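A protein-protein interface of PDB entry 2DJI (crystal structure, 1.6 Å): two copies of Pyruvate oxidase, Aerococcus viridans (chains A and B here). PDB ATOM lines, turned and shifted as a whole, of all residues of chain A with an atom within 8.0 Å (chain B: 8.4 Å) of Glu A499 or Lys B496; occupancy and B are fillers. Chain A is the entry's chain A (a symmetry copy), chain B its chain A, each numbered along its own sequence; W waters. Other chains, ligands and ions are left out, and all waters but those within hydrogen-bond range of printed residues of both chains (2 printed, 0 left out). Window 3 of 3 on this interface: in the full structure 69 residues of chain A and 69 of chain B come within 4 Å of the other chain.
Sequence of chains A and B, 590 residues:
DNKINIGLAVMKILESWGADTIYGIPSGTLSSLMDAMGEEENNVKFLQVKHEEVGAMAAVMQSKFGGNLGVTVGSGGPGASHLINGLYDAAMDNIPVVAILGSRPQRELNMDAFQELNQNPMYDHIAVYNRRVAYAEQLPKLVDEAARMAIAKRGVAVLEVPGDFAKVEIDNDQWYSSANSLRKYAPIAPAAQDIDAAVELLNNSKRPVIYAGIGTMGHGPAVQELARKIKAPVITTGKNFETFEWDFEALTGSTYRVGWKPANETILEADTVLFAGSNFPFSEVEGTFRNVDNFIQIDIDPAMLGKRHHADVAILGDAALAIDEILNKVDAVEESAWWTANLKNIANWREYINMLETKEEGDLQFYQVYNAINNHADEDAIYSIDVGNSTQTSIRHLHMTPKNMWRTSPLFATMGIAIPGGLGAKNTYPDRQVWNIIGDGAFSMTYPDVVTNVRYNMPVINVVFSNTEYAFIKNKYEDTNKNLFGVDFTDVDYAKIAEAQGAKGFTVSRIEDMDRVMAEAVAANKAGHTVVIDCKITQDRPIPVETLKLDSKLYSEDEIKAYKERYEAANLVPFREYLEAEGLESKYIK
O of Ala A500 lies within hydrogen-bond range of N of Asp B493. The backbone carbonyl oxygen (O) of Ala B500 is in hydrogen-bond range of the backbone NH (N) of Asp A493 (3.0 Å).
Water W1 lies within hydrogen-bond range of NZ of Lys A496 (2.6 Å) and O of Glu B499 (3.3 Å). Water W2 lies within hydrogen-bond range of the side-chain amino group of Lys B496 (2.6 Å) and the backbone carbonyl oxygen of Glu A499 (3.3 Å).
Hydrophobic or aromatic side chains of chain A within 4 Å of the printed part of chain B: Ile A497 and Ala A500. Of the 19 printed residues of chain B, 6 touch a printed residue of chain A. Hydrophobic or aromatic side chains of chain B within 4 Å of the printed part of chain A: Val B492, Ile B497 and Ala B500. Among the printed residues, 10 pairs touch across the chains. Among the printed residues, no Asp or Glu carboxylate lies within 4 Å of a Lys or Arg side-chain nitrogen of the other chain.
Asp A493 touches Ala B500, and with the chains exchanged Ala A500 touches Asp B493. Lys B496 touches its own counterpart, Lys A496. Lys A496 touches Glu B499, and with the chains exchanged Glu A499 touches Lys B496. Lys A496 touches Ala B500, and with the chains exchanged Ala A500 touches Lys B496.
CE of Lys A496 touches CG of Lys B496, 3.4 Å away. Lys A496 touches Glu B499. Lys A496 touches Ala B500. Ala B500 touches Ile A497 (CB to CG1, 3.6 Å). Lys B496 touches Glu A499 (NZ to CB, 3.2 Å). CA of Val B492 touches O of Ala A500 (3.5 Å). Lys B496 touches Ala A500 (CD to CB, 3.8 Å). Ile B497 touches Ala A500 (CG1 to CB, 3.6 Å).
The side-chain carboxylate of Asp B493 sits close to the backbone NH of Ala B495, at 3.2 Å. OD1 of Asp A493 sits close to N of Ala A495. The backbone NH (N) of Gly B505 sits at hydrogen-bond distance from the side-chain carboxylate (OE1) of Glu B499, at 2.9 Å. The side-chain carboxylate (OE1) of Glu A499 is in hydrogen-bond range of the backbone NH (N) of Gly A505, 2.9 Å away. The side-chain carboxylate of Asp A493 lies within hydrogen-bond range of the backbone NH of Lys A496, at 3.0 Å. OD1 of Asp B493 sits at hydrogen-bond distance from N of Lys B496 (3.0 Å).
Of the printed residues of chain B, Lys A496 touches Lys B496 (3.4 Å), Glu B499 (3.2 Å) and Ala B500 (3.8 Å). Of chain B, only Lys B496 (3.2 Å) comes within 4 Å of Glu A499. Ala A500 touches just these residues of chain B: Val B492 (3.5 Å), Asp B493 (3.0 Å), Lys B496 (3.8 Å) and Ile B497 (3.6 Å). No residue of chain B comes within 4 Å of Gly A505. Printed residues of chain A within 4 Å of Val B492: Ala A500 (3.5 Å). Of the printed residues of chain A, Asp B493 touches Ala A500 (3.0 Å). No residue of chain A comes within 4 Å of Ala B495. Printed residues of chain A within 4 Å of Ile B497: Ala A500. Ala B498 touches none of the printed residues of chain A. Printed residues of chain A within 4 Å of Glu B499: Lys A496 (3.2 Å). The nearest residue of chain A that does not touch Lys B496 is Ile A497 (5.5 Å). The nearest printed residue of chain A that does not touch Ile B497 is Ile A497 (4.2 Å).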
ATOM      1  N   VAL A 450      17.651  -1.546  18.803  1.00  0.00           N
ATOM      2  CA  VAL A 450      18.764  -0.631  19.003  1.00  0.00           C
ATOM      3  C   VAL A 450      19.428  -1.083  20.303  1.00  0.00           C
ATOM      4  O   VAL A 450      20.641  -0.959  20.476  1.00  0.00           O
ATOM      5  CB  VAL A 450      18.272   0.824  19.158  1.00  0.00           C
ATOM      6  CG1 VAL A 450      19.379   1.701  19.750  1.00  0.00           C
ATOM      7  CG2 VAL A 450      17.846   1.365  17.802  1.00  0.00           C
ATOM      8  N   VAL A 454      23.454  -1.845  21.995  1.00  0.00           N
ATOM      9  CA  VAL A 454      23.863  -1.379  23.314  1.00  0.00           C
ATOM     10  C   VAL A 454      24.341  -2.543  24.178  1.00  0.00           C
ATOM     11  O   VAL A 454      25.463  -2.534  24.686  1.00  0.00           O
ATOM     12  CB  VAL A 454      22.694  -0.671  24.042  1.00  0.00           C
ATOM     13  CG1 VAL A 454      23.102  -0.310  25.467  1.00  0.00           C
ATOM     14  CG2 VAL A 454      22.289   0.580  23.279  1.00  0.00           C
ATOM     15  N   ASP A 493       9.393  10.852  19.457  1.00  0.00           N
ATOM     16  CA  ASP A 493      10.701  11.355  19.877  1.00  0.00           C
ATOM     17  C   ASP A 493      11.706  10.203  19.892  1.00  0.00           C
ATOM     18  O   ASP A 493      11.914   9.562  20.924  1.00  0.00           O
ATOM     19  CB  ASP A 493      10.598  11.959  21.281  1.00  0.00           C
ATOM     20  CG  ASP A 493      11.845  12.726  21.682  1.00  0.00           C
ATOM     21  OD1 ASP A 493      12.936  12.439  21.141  1.00  0.00           O
ATOM     22  OD2 ASP A 493      11.731  13.613  22.556  1.00  0.00           O
ATOM     23  N   TYR A 494      12.331   9.944  18.749  1.00  0.00           N
ATOM     24  CA  TYR A 494      13.291   8.851  18.648  1.00  0.00           C
ATOM     25  C   TYR A 494      14.528   9.032  19.518  1.00  0.00           C
ATOM     26  O   TYR A 494      15.122   8.049  19.960  1.00  0.00           O
ATOM     27  CB  TYR A 494      13.700   8.639  17.187  1.00  0.00           C
ATOM     28  CG  TYR A 494      12.537   8.269  16.300  1.00  0.00           C
ATOM     29  CD1 TYR A 494      12.184   9.064  15.212  1.00  0.00           C
ATOM     30  CD2 TYR A 494      11.761   7.142  16.572  1.00  0.00           C
ATOM     31  CE1 TYR A 494      11.081   8.750  14.419  1.00  0.00           C
ATOM     32  CE2 TYR A 494      10.659   6.819  15.788  1.00  0.00           C
ATOM     33  CZ  TYR A 494      10.322   7.627  14.715  1.00  0.00           C
ATOM     34  OH  TYR A 494       9.212   7.330  13.957  1.00  0.00           O
ATOM     35  N   ALA A 495      14.918  10.278  19.769  1.00  0.00           N
ATOM     36  CA  ALA A 495      16.081  10.542  20.606  1.00  0.00           C
ATOM     37  C   ALA A 495      15.799  10.070  22.031  1.00  0.00           C
ATOM     38  O   ALA A 495      16.653   9.466  22.683  1.00  0.00           O
ATOM     39  CB  ALA A 495      16.409  12.034  20.602  1.00  0.00           C
ATOM     40  N   LYS A 496      14.587  10.342  22.503  1.00  0.00           N
ATOM     41  CA  LYS A 496      14.180   9.951  23.848  1.00  0.00           C
ATOM     42  C   LYS A 496      14.110   8.429  23.964  1.00  0.00           C
ATOM     43  O   LYS A 496      14.495   7.850  24.982  1.00  0.00           O
ATOM     44  CB  LYS A 496      12.819  10.573  24.179  1.00  0.00           C
ATOM     45  CG  LYS A 496      12.329  10.280  25.582  1.00  0.00           C
ATOM     46  CD  LYS A 496      11.104  11.111  25.926  1.00  0.00           C
ATOM     47  CE  LYS A 496      10.614  10.808  27.334  1.00  0.00           C
ATOM     48  NZ  LYS A 496       9.479  11.688  27.729  1.00  0.00           N
ATOM     49  N   ILE A 497      13.611   7.781  22.919  1.00  0.00           N
ATOM     50  CA  ILE A 497      13.521   6.327  22.921  1.00  0.00           C
ATOM     51  C   ILE A 497      14.931   5.755  23.029  1.00  0.00           C
ATOM     52  O   ILE A 497      15.181   4.828  23.801  1.00  0.00           O
ATOM     53  CB  ILE A 497      12.839   5.816  21.636  1.00  0.00           C
ATOM     54  CG1 ILE A 497      11.371   6.258  21.639  1.00  0.00           C
ATOM     55  CG2 ILE A 497      12.959   4.289  21.544  1.00  0.00           C
ATOM     56  CD1 ILE A 497      10.594   5.868  20.396  1.00  0.00           C
ATOM     57  N   ALA A 498      15.855   6.324  22.261  1.00  0.00           N
ATOM     58  CA  ALA A 498      17.238   5.869  22.281  1.00  0.00           C
ATOM     59  C   ALA A 498      17.800   5.940  23.700  1.00  0.00           C
ATOM     60  O   ALA A 498      18.450   5.005  24.165  1.00  0.00           O
ATOM     61  CB  ALA A 498      18.081   6.717  21.337  1.00  0.00           C
ATOM     62  N   GLU A 499      17.545   7.051  24.385  1.00  0.00           N
ATOM     63  CA  GLU A 499      18.030   7.225  25.749  1.00  0.00           C
ATOM     64  C   GLU A 499      17.451   6.157  26.664  1.00  0.00           C
ATOM     65  O   GLU A 499      18.153   5.604  27.508  1.00  0.00           O
ATOM     66  CB  GLU A 499      17.646   8.610  26.275  1.00  0.00           C
ATOM     67  CG  GLU A 499      18.341   9.754  25.558  1.00  0.00           C
ATOM     68  CD  GLU A 499      19.809   9.875  25.929  1.00  0.00           C
ATOM     69  OE1 GLU A 499      20.568  10.506  25.163  1.00  0.00           O
ATOM     70  OE2 GLU A 499      20.204   9.352  26.994  1.00  0.00           O
ATOM     71  N   ALA A 500      16.167   5.869  26.489  1.00  0.00           N
ATOM     72  CA  ALA A 500      15.496   4.864  27.304  1.00  0.00           C
ATOM     73  C   ALA A 500      16.089   3.477  27.079  1.00  0.00           C
ATOM     74  O   ALA A 500      15.949   2.593  27.924  1.00  0.00           O
ATOM     75  CB  ALA A 500      14.004   4.850  26.989  1.00  0.00           C
ATOM     76  N   GLN A 501      16.761   3.296  25.943  1.00  0.00           N
ATOM     77  CA  GLN A 501      17.364   2.013  25.588  1.00  0.00           C
ATOM     78  C   GLN A 501      18.838   1.907  25.957  1.00  0.00           C
ATOM     79  O   GLN A 501      19.464   0.871  25.730  1.00  0.00           O
ATOM     80  CB  GLN A 501      17.224   1.770  24.083  1.00  0.00           C
ATOM     81  CG  GLN A 501      15.800   1.799  23.573  1.00  0.00           C
ATOM     82  CD  GLN A 501      15.742   1.769  22.063  1.00  0.00           C
ATOM     83  OE1 GLN A 501      16.379   2.584  21.391  1.00  0.00           O
ATOM     84  NE2 GLN A 501      14.976   0.833  21.517  1.00  0.00           N
ATOM     85  N   GLY A 502      19.400   2.978  26.508  1.00  0.00           N
ATOM     86  CA  GLY A 502      20.805   2.952  26.876  1.00  0.00           C
ATOM     87  C   GLY A 502      21.701   3.507  25.784  1.00  0.00           C
ATOM     88  O   GLY A 502      22.927   3.418  25.867  1.00  0.00           O
ATOM     89  N   ALA A 503      21.090   4.072  24.748  1.00  0.00           N
ATOM     90  CA  ALA A 503      21.841   4.660  23.647  1.00  0.00           C
ATOM     91  C   ALA A 503      21.835   6.171  23.835  1.00  0.00           C
ATOM     92  O   ALA A 503      21.148   6.687  24.716  1.00  0.00           O
ATOM     93  CB  ALA A 503      21.199   4.292  22.310  1.00  0.00           C
ATOM     94  N   LYS A 504      22.607   6.877  23.019  1.00  0.00           N
ATOM     95  CA  LYS A 504      22.663   8.329  23.104  1.00  0.00           C
ATOM     96  C   LYS A 504      21.825   8.918  21.980  1.00  0.00           C
ATOM     97  O   LYS A 504      22.048   8.615  20.809  1.00  0.00           O
ATOM     98  CB  LYS A 504      24.111   8.811  22.987  1.00  0.00           C
ATOM     99  CG  LYS A 504      24.264  10.317  22.846  1.00  0.00           C
ATOM    100  CD  LYS A 504      23.703  11.081  24.034  1.00  0.00           C
ATOM    101  CE  LYS A 504      23.903  12.582  23.850  1.00  0.00           C
ATOM    102  NZ  LYS A 504      23.394  13.379  25.005  1.00  0.00           N
ATOM    103  N   GLY A 505      20.859   9.757  22.339  1.00  0.00           N
ATOM    104  CA  GLY A 505      20.004  10.353  21.330  1.00  0.00           C
ATOM    105  C   GLY A 505      20.252  11.825  21.064  1.00  0.00           C
ATOM    106  O   GLY A 505      20.589  12.592  21.972  1.00  0.00           O
ATOM    107  N   PHE A 506      20.097  12.209  19.801  1.00  0.00           N
ATOM    108  CA  PHE A 506      20.267  13.591  19.370  1.00  0.00           C
ATOM    109  C   PHE A 506      19.077  13.958  18.501  1.00  0.00           C
ATOM    110  O   PHE A 506      18.488  13.097  17.847  1.00  0.00           O
ATOM    111  CB  PHE A 506      21.544  13.768  18.539  1.00  0.00           C
ATOM    112  CG  PHE A 506      22.806  13.428  19.272  1.00  0.00           C
ATOM    113  CD1 PHE A 506      23.231  12.109  19.376  1.00  0.00           C
ATOM    114  CD2 PHE A 506      23.577  14.430  19.855  1.00  0.00           C
ATOM    115  CE1 PHE A 506      24.405  11.791  20.047  1.00  0.00           C
ATOM    116  CE2 PHE A 506      24.753  14.123  20.529  1.00  0.00           C
ATOM    117  CZ  PHE A 506      25.170  12.802  20.626  1.00  0.00           C
ATOM    118  N   HIS A 529      29.419   4.506  22.532  1.00  0.00           N
ATOM    119  CA  HIS A 529      27.962   4.564  22.599  1.00  0.00           C
ATOM    120  C   HIS A 529      27.290   4.338  21.253  1.00  0.00           C
ATOM    121  O   HIS A 529      27.809   4.734  20.211  1.00  0.00           O
ATOM    122  CB  HIS A 529      27.492   5.926  23.125  1.00  0.00           C
ATOM    123  CG  HIS A 529      27.795   6.163  24.571  1.00  0.00           C
ATOM    124  ND1 HIS A 529      29.075   6.366  25.041  1.00  0.00           N
ATOM    125  CD2 HIS A 529      26.980   6.243  25.649  1.00  0.00           C
ATOM    126  CE1 HIS A 529      29.035   6.564  26.346  1.00  0.00           C
ATOM    127  NE2 HIS A 529      27.776   6.495  26.740  1.00  0.00           N
ATOM    128  N   THR A 530      26.142   3.672  21.280  1.00  0.00           N
ATOM    129  CA  THR A 530      25.366   3.498  20.068  1.00  0.00           C
ATOM    130  C   THR A 530      24.604   4.813  20.061  1.00  0.00           C
ATOM    131  O   THR A 530      24.167   5.284  21.110  1.00  0.00           O
ATOM    132  CB  THR A 530      24.384   2.318  20.173  1.00  0.00           C
ATOM    133  OG1 THR A 530      25.101   1.095  19.988  1.00  0.00           O
ATOM    134  CG2 THR A 530      23.286   2.430  19.116  1.00  0.00           C
ATOM    135  N   VAL A 532      21.650   7.582  18.122  1.00  0.00           N
ATOM    136  CA  VAL A 532      20.489   7.734  17.264  1.00  0.00           C
ATOM    137  C   VAL A 532      20.332   9.225  17.024  1.00  0.00           C
ATOM    138  O   VAL A 532      20.133   9.999  17.965  1.00  0.00           O
ATOM    139  CB  VAL A 532      19.195   7.201  17.918  1.00  0.00           C
ATOM    140  CG1 VAL A 532      17.998   7.496  17.016  1.00  0.00           C
ATOM    141  CG2 VAL A 532      19.312   5.702  18.155  1.00  0.00           C
ATOM    142  N   ASP B 491      17.864  -3.277  31.144  1.00  0.00           N
ATOM    143  CA  ASP B 491      16.573  -2.788  31.615  1.00  0.00           C
ATOM    144  C   ASP B 491      16.138  -1.503  30.916  1.00  0.00           C
ATOM    145  O   ASP B 491      16.461  -0.396  31.347  1.00  0.00           O
ATOM    146  CB  ASP B 491      16.608  -2.562  33.128  1.00  0.00           C
ATOM    147  CG  ASP B 491      15.230  -2.298  33.705  1.00  0.00           C
ATOM    148  OD1 ASP B 491      14.336  -3.152  33.521  1.00  0.00           O
ATOM    149  OD2 ASP B 491      15.039  -1.240  34.340  1.00  0.00           O
ATOM    150  N   VAL B 492      15.391  -1.670  29.832  1.00  0.00           N
ATOM    151  CA  VAL B 492      14.889  -0.554  29.046  1.00  0.00           C
ATOM    152  C   VAL B 492      13.779   0.183  29.796  1.00  0.00           C
ATOM    153  O   VAL B 492      12.956  -0.439  30.469  1.00  0.00           O
ATOM    154  CB  VAL B 492      14.355  -1.061  27.689  1.00  0.00           C
ATOM    155  CG1 VAL B 492      13.727   0.072  26.910  1.00  0.00           C
ATOM    156  CG2 VAL B 492      15.498  -1.685  26.895  1.00  0.00           C
ATOM    157  N   ASP B 493      13.769   1.507  29.684  1.00  0.00           N
ATOM    158  CA  ASP B 493      12.761   2.333  30.350  1.00  0.00           C
ATOM    159  C   ASP B 493      11.516   2.422  29.468  1.00  0.00           C
ATOM    160  O   ASP B 493      11.374   3.353  28.673  1.00  0.00           O
ATOM    161  CB  ASP B 493      13.318   3.740  30.589  1.00  0.00           C
ATOM    162  CG  ASP B 493      12.434   4.574  31.497  1.00  0.00           C
ATOM    163  OD1 ASP B 493      11.216   4.299  31.579  1.00  0.00           O
ATOM    164  OD2 ASP B 493      12.962   5.520  32.120  1.00  0.00           O
ATOM    165  N   TYR B 494      10.614   1.458  29.611  1.00  0.00           N
ATOM    166  CA  TYR B 494       9.402   1.435  28.800  1.00  0.00           C
ATOM    167  C   TYR B 494       8.474   2.618  29.043  1.00  0.00           C
ATOM    168  O   TYR B 494       7.751   3.033  28.138  1.00  0.00           O
ATOM    169  CB  TYR B 494       8.648   0.119  29.012  1.00  0.00           C
ATOM    170  CG  TYR B 494       9.454  -1.091  28.609  1.00  0.00           C
ATOM    171  CD1 TYR B 494       9.762  -2.088  29.532  1.00  0.00           C
ATOM    172  CD2 TYR B 494       9.945  -1.221  27.309  1.00  0.00           C
ATOM    173  CE1 TYR B 494      10.546  -3.184  29.173  1.00  0.00           C
ATOM    174  CE2 TYR B 494      10.729  -2.309  26.941  1.00  0.00           C
ATOM    175  CZ  TYR B 494      11.028  -3.285  27.876  1.00  0.00           C
ATOM    176  OH  TYR B 494      11.830  -4.346  27.525  1.00  0.00           O
ATOM    177  N   ALA B 495       8.488   3.162  30.257  1.00  0.00           N
ATOM    178  CA  ALA B 495       7.644   4.308  30.571  1.00  0.00           C
ATOM    179  C   ALA B 495       8.091   5.511  29.743  1.00  0.00           C
ATOM    180  O   ALA B 495       7.269   6.256  29.207  1.00  0.00           O
ATOM    181  CB  ALA B 495       7.727   4.634  32.061  1.00  0.00           C
ATOM    182  N   LYS B 496       9.404   5.686  29.636  1.00  0.00           N
ATOM    183  CA  LYS B 496       9.973   6.793  28.877  1.00  0.00           C
ATOM    184  C   LYS B 496       9.663   6.636  27.389  1.00  0.00           C
ATOM    185  O   LYS B 496       9.368   7.610  26.694  1.00  0.00           O
ATOM    186  CB  LYS B 496      11.487   6.852  29.102  1.00  0.00           C
ATOM    187  CG  LYS B 496      12.173   8.009  28.404  1.00  0.00           C
ATOM    188  CD  LYS B 496      13.617   8.150  28.854  1.00  0.00           C
ATOM    189  CE  LYS B 496      14.302   9.310  28.147  1.00  0.00           C
ATOM    190  NZ  LYS B 496      15.686   9.531  28.652  1.00  0.00           N
ATOM    191  N   ILE B 497       9.738   5.405  26.898  1.00  0.00           N
ATOM    192  CA  ILE B 497       9.440   5.145  25.496  1.00  0.00           C
ATOM    193  C   ILE B 497       7.987   5.525  25.231  1.00  0.00           C
ATOM    194  O   ILE B 497       7.673   6.173  24.231  1.00  0.00           O
ATOM    195  CB  ILE B 497       9.671   3.661  25.150  1.00  0.00           C
ATOM    196  CG1 ILE B 497      11.169   3.350  25.255  1.00  0.00           C
ATOM    197  CG2 ILE B 497       9.137   3.354  23.745  1.00  0.00           C
ATOM    198  CD1 ILE B 497      11.530   1.900  24.995  1.00  0.00           C
ATOM    199  N   ALA B 498       7.103   5.131  26.142  1.00  0.00           N
ATOM    200  CA  ALA B 498       5.686   5.440  26.002  1.00  0.00           C
ATOM    201  C   ALA B 498       5.481   6.948  25.874  1.00  0.00           C
ATOM    202  O   ALA B 498       4.724   7.408  25.021  1.00  0.00           O
ATOM    203  CB  ALA B 498       4.914   4.903  27.201  1.00  0.00           C
ATOM    204  N   GLU B 499       6.161   7.714  26.722  1.00  0.00           N
ATOM    205  CA  GLU B 499       6.044   9.167  26.688  1.00  0.00           C
ATOM    206  C   GLU B 499       6.503   9.709  25.344  1.00  0.00           C
ATOM    207  O   GLU B 499       5.879  10.607  24.780  1.00  0.00           O
ATOM    208  CB  GLU B 499       6.882   9.793  27.805  1.00  0.00           C
ATOM    209  CG  GLU B 499       6.375   9.481  29.201  1.00  0.00           C
ATOM    210  CD  GLU B 499       5.106  10.240  29.550  1.00  0.00           C
ATOM    211  OE1 GLU B 499       4.393   9.814  30.484  1.00  0.00           O
ATOM    212  OE2 GLU B 499       4.826  11.271  28.900  1.00  0.00           O
ATOM    213  N   ALA B 500       7.598   9.158  24.833  1.00  0.00           N
ATOM    214  CA  ALA B 500       8.140   9.592  23.551  1.00  0.00           C
ATOM    215  C   ALA B 500       7.169   9.308  22.410  1.00  0.00           C
ATOM    216  O   ALA B 500       7.250   9.929  21.351  1.00  0.00           O
ATOM    217  CB  ALA B 500       9.472   8.899  23.288  1.00  0.00           C
ATOM    218  N   GLN B 501       6.245   8.375  22.636  1.00  0.00           N
ATOM    219  CA  GLN B 501       5.265   7.985  21.626  1.00  0.00           C
ATOM    220  C   GLN B 501       3.929   8.707  21.758  1.00  0.00           C
ATOM    221  O   GLN B 501       3.020   8.485  20.959  1.00  0.00           O
ATOM    222  CB  GLN B 501       5.009   6.478  21.699  1.00  0.00           C
ATOM    223  CG  GLN B 501       6.246   5.623  21.535  1.00  0.00           C
ATOM    224  CD  GLN B 501       5.968   4.167  21.831  1.00  0.00           C
ATOM    225  OE1 GLN B 501       5.439   3.829  22.893  1.00  0.00           O
ATOM    226  NE2 GLN B 501       6.325   3.293  20.899  1.00  0.00           N
ATOM    227  N   GLY B 502       3.801   9.554  22.775  1.00  0.00           N
ATOM    228  CA  GLY B 502       2.552  10.268  22.970  1.00  0.00           C
ATOM    229  C   GLY B 502       1.620   9.558  23.934  1.00  0.00           C
ATOM    230  O   GLY B 502       0.461   9.944  24.094  1.00  0.00           O
ATOM    231  N   ALA B 503       2.121   8.504  24.571  1.00  0.00           N
ATOM    232  CA  ALA B 503       1.332   7.751  25.537  1.00  0.00           C
ATOM    233  C   ALA B 503       1.776   8.176  26.930  1.00  0.00           C
ATOM    234  O   ALA B 503       2.747   8.917  27.077  1.00  0.00           O
ATOM    235  CB  ALA B 503       1.552   6.250  25.347  1.00  0.00           C
ATOM    236  N   LYS B 504       1.061   7.718  27.950  1.00  0.00           N
ATOM    237  CA  LYS B 504       1.408   8.051  29.323  1.00  0.00           C
ATOM    238  C   LYS B 504       2.109   6.858  29.954  1.00  0.00           C
ATOM    239  O   LYS B 504       1.568   5.754  29.976  1.00  0.00           O
ATOM    240  CB  LYS B 504       0.147   8.400  30.119  1.00  0.00           C
ATOM    241  CG  LYS B 504       0.369   8.553  31.615  1.00  0.00           C
ATOM    242  CD  LYS B 504       1.353   9.660  31.956  1.00  0.00           C
ATOM    243  CE  LYS B 504       1.520   9.783  33.467  1.00  0.00           C
ATOM    244  NZ  LYS B 504       2.456  10.878  33.858  1.00  0.00           N
ATOM    245  N   GLY B 505       3.316   7.084  30.465  1.00  0.00           N
ATOM    246  CA  GLY B 505       4.059   5.997  31.073  1.00  0.00           C
ATOM    247  C   GLY B 505       4.156   6.050  32.584  1.00  0.00           C
ATOM    248  O   GLY B 505       4.236   7.127  33.184  1.00  0.00           O
ATOM    249  N   PHE B 506       4.132   4.871  33.199  1.00  0.00           N
ATOM    250  CA  PHE B 506       4.243   4.732  34.645  1.00  0.00           C
ATOM    251  C   PHE B 506       5.272   3.653  34.932  1.00  0.00           C
ATOM    252  O   PHE B 506       5.459   2.735  34.133  1.00  0.00           O
ATOM    253  CB  PHE B 506       2.910   4.307  35.273  1.00  0.00           C
ATOM    254  CG  PHE B 506       1.791   5.280  35.057  1.00  0.00           C
ATOM    255  CD1 PHE B 506       1.067   5.275  33.871  1.00  0.00           C
ATOM    256  CD2 PHE B 506       1.455   6.202  36.046  1.00  0.00           C
ATOM    257  CE1 PHE B 506       0.023   6.170  33.672  1.00  0.00           C
ATOM    258  CE2 PHE B 506       0.413   7.102  35.856  1.00  0.00           C
ATOM    259  CZ  PHE B 506      -0.306   7.087  34.668  1.00  0.00           C
ATOM    260  N   THR B 507       5.938   3.768  36.074  1.00  0.00           N
ATOM    261  CA  THR B 507       6.936   2.792  36.480  1.00  0.00           C
ATOM    262  C   THR B 507       6.647   2.420  37.928  1.00  0.00           C
ATOM    263  O   THR B 507       6.444   3.290  38.771  1.00  0.00           O
ATOM    264  CB  THR B 507       8.363   3.368  36.384  1.00  0.00           C
ATOM    265  OG1 THR B 507       8.607   3.824  35.046  1.00  0.00           O
ATOM    266  CG2 THR B 507       9.393   2.304  36.740  1.00  0.00           C
ATOM    267  N   VAL B 532       1.094   2.926  29.508  1.00  0.00           N
ATOM    268  CA  VAL B 532       2.041   1.830  29.594  1.00  0.00           C
ATOM    269  C   VAL B 532       2.530   1.805  31.031  1.00  0.00           C
ATOM    270  O   VAL B 532       3.122   2.773  31.515  1.00  0.00           O
ATOM    271  CB  VAL B 532       3.258   2.024  28.663  1.00  0.00           C
ATOM    272  CG1 VAL B 532       4.268   0.900  28.888  1.00  0.00           C
ATOM    273  CG2 VAL B 532       2.805   2.034  27.210  1.00  0.00           C
ATOM    274  N   ASP B 534       5.063   0.123  33.313  1.00  0.00           N
ATOM    275  CA  ASP B 534       6.271  -0.690  33.332  1.00  0.00           C
ATOM    276  C   ASP B 534       6.389  -1.263  34.735  1.00  0.00           C
ATOM    277  O   ASP B 534       6.812  -0.575  35.665  1.00  0.00           O
ATOM    278  CB  ASP B 534       7.493   0.172  33.001  1.00  0.00           C
ATOM    279  CG  ASP B 534       8.769  -0.643  32.859  1.00  0.00           C
ATOM    280  OD1 ASP B 534       8.735  -1.872  33.081  1.00  0.00           O
ATOM    281  OD2 ASP B 534       9.812  -0.050  32.524  1.00  0.00           O
HETATM  282  O   HOH W   1       8.153  12.849  25.760  1.00  0.00           O
HETATM  283  O   HOH W   2      16.814   7.500  29.911  1.00  0.00           O
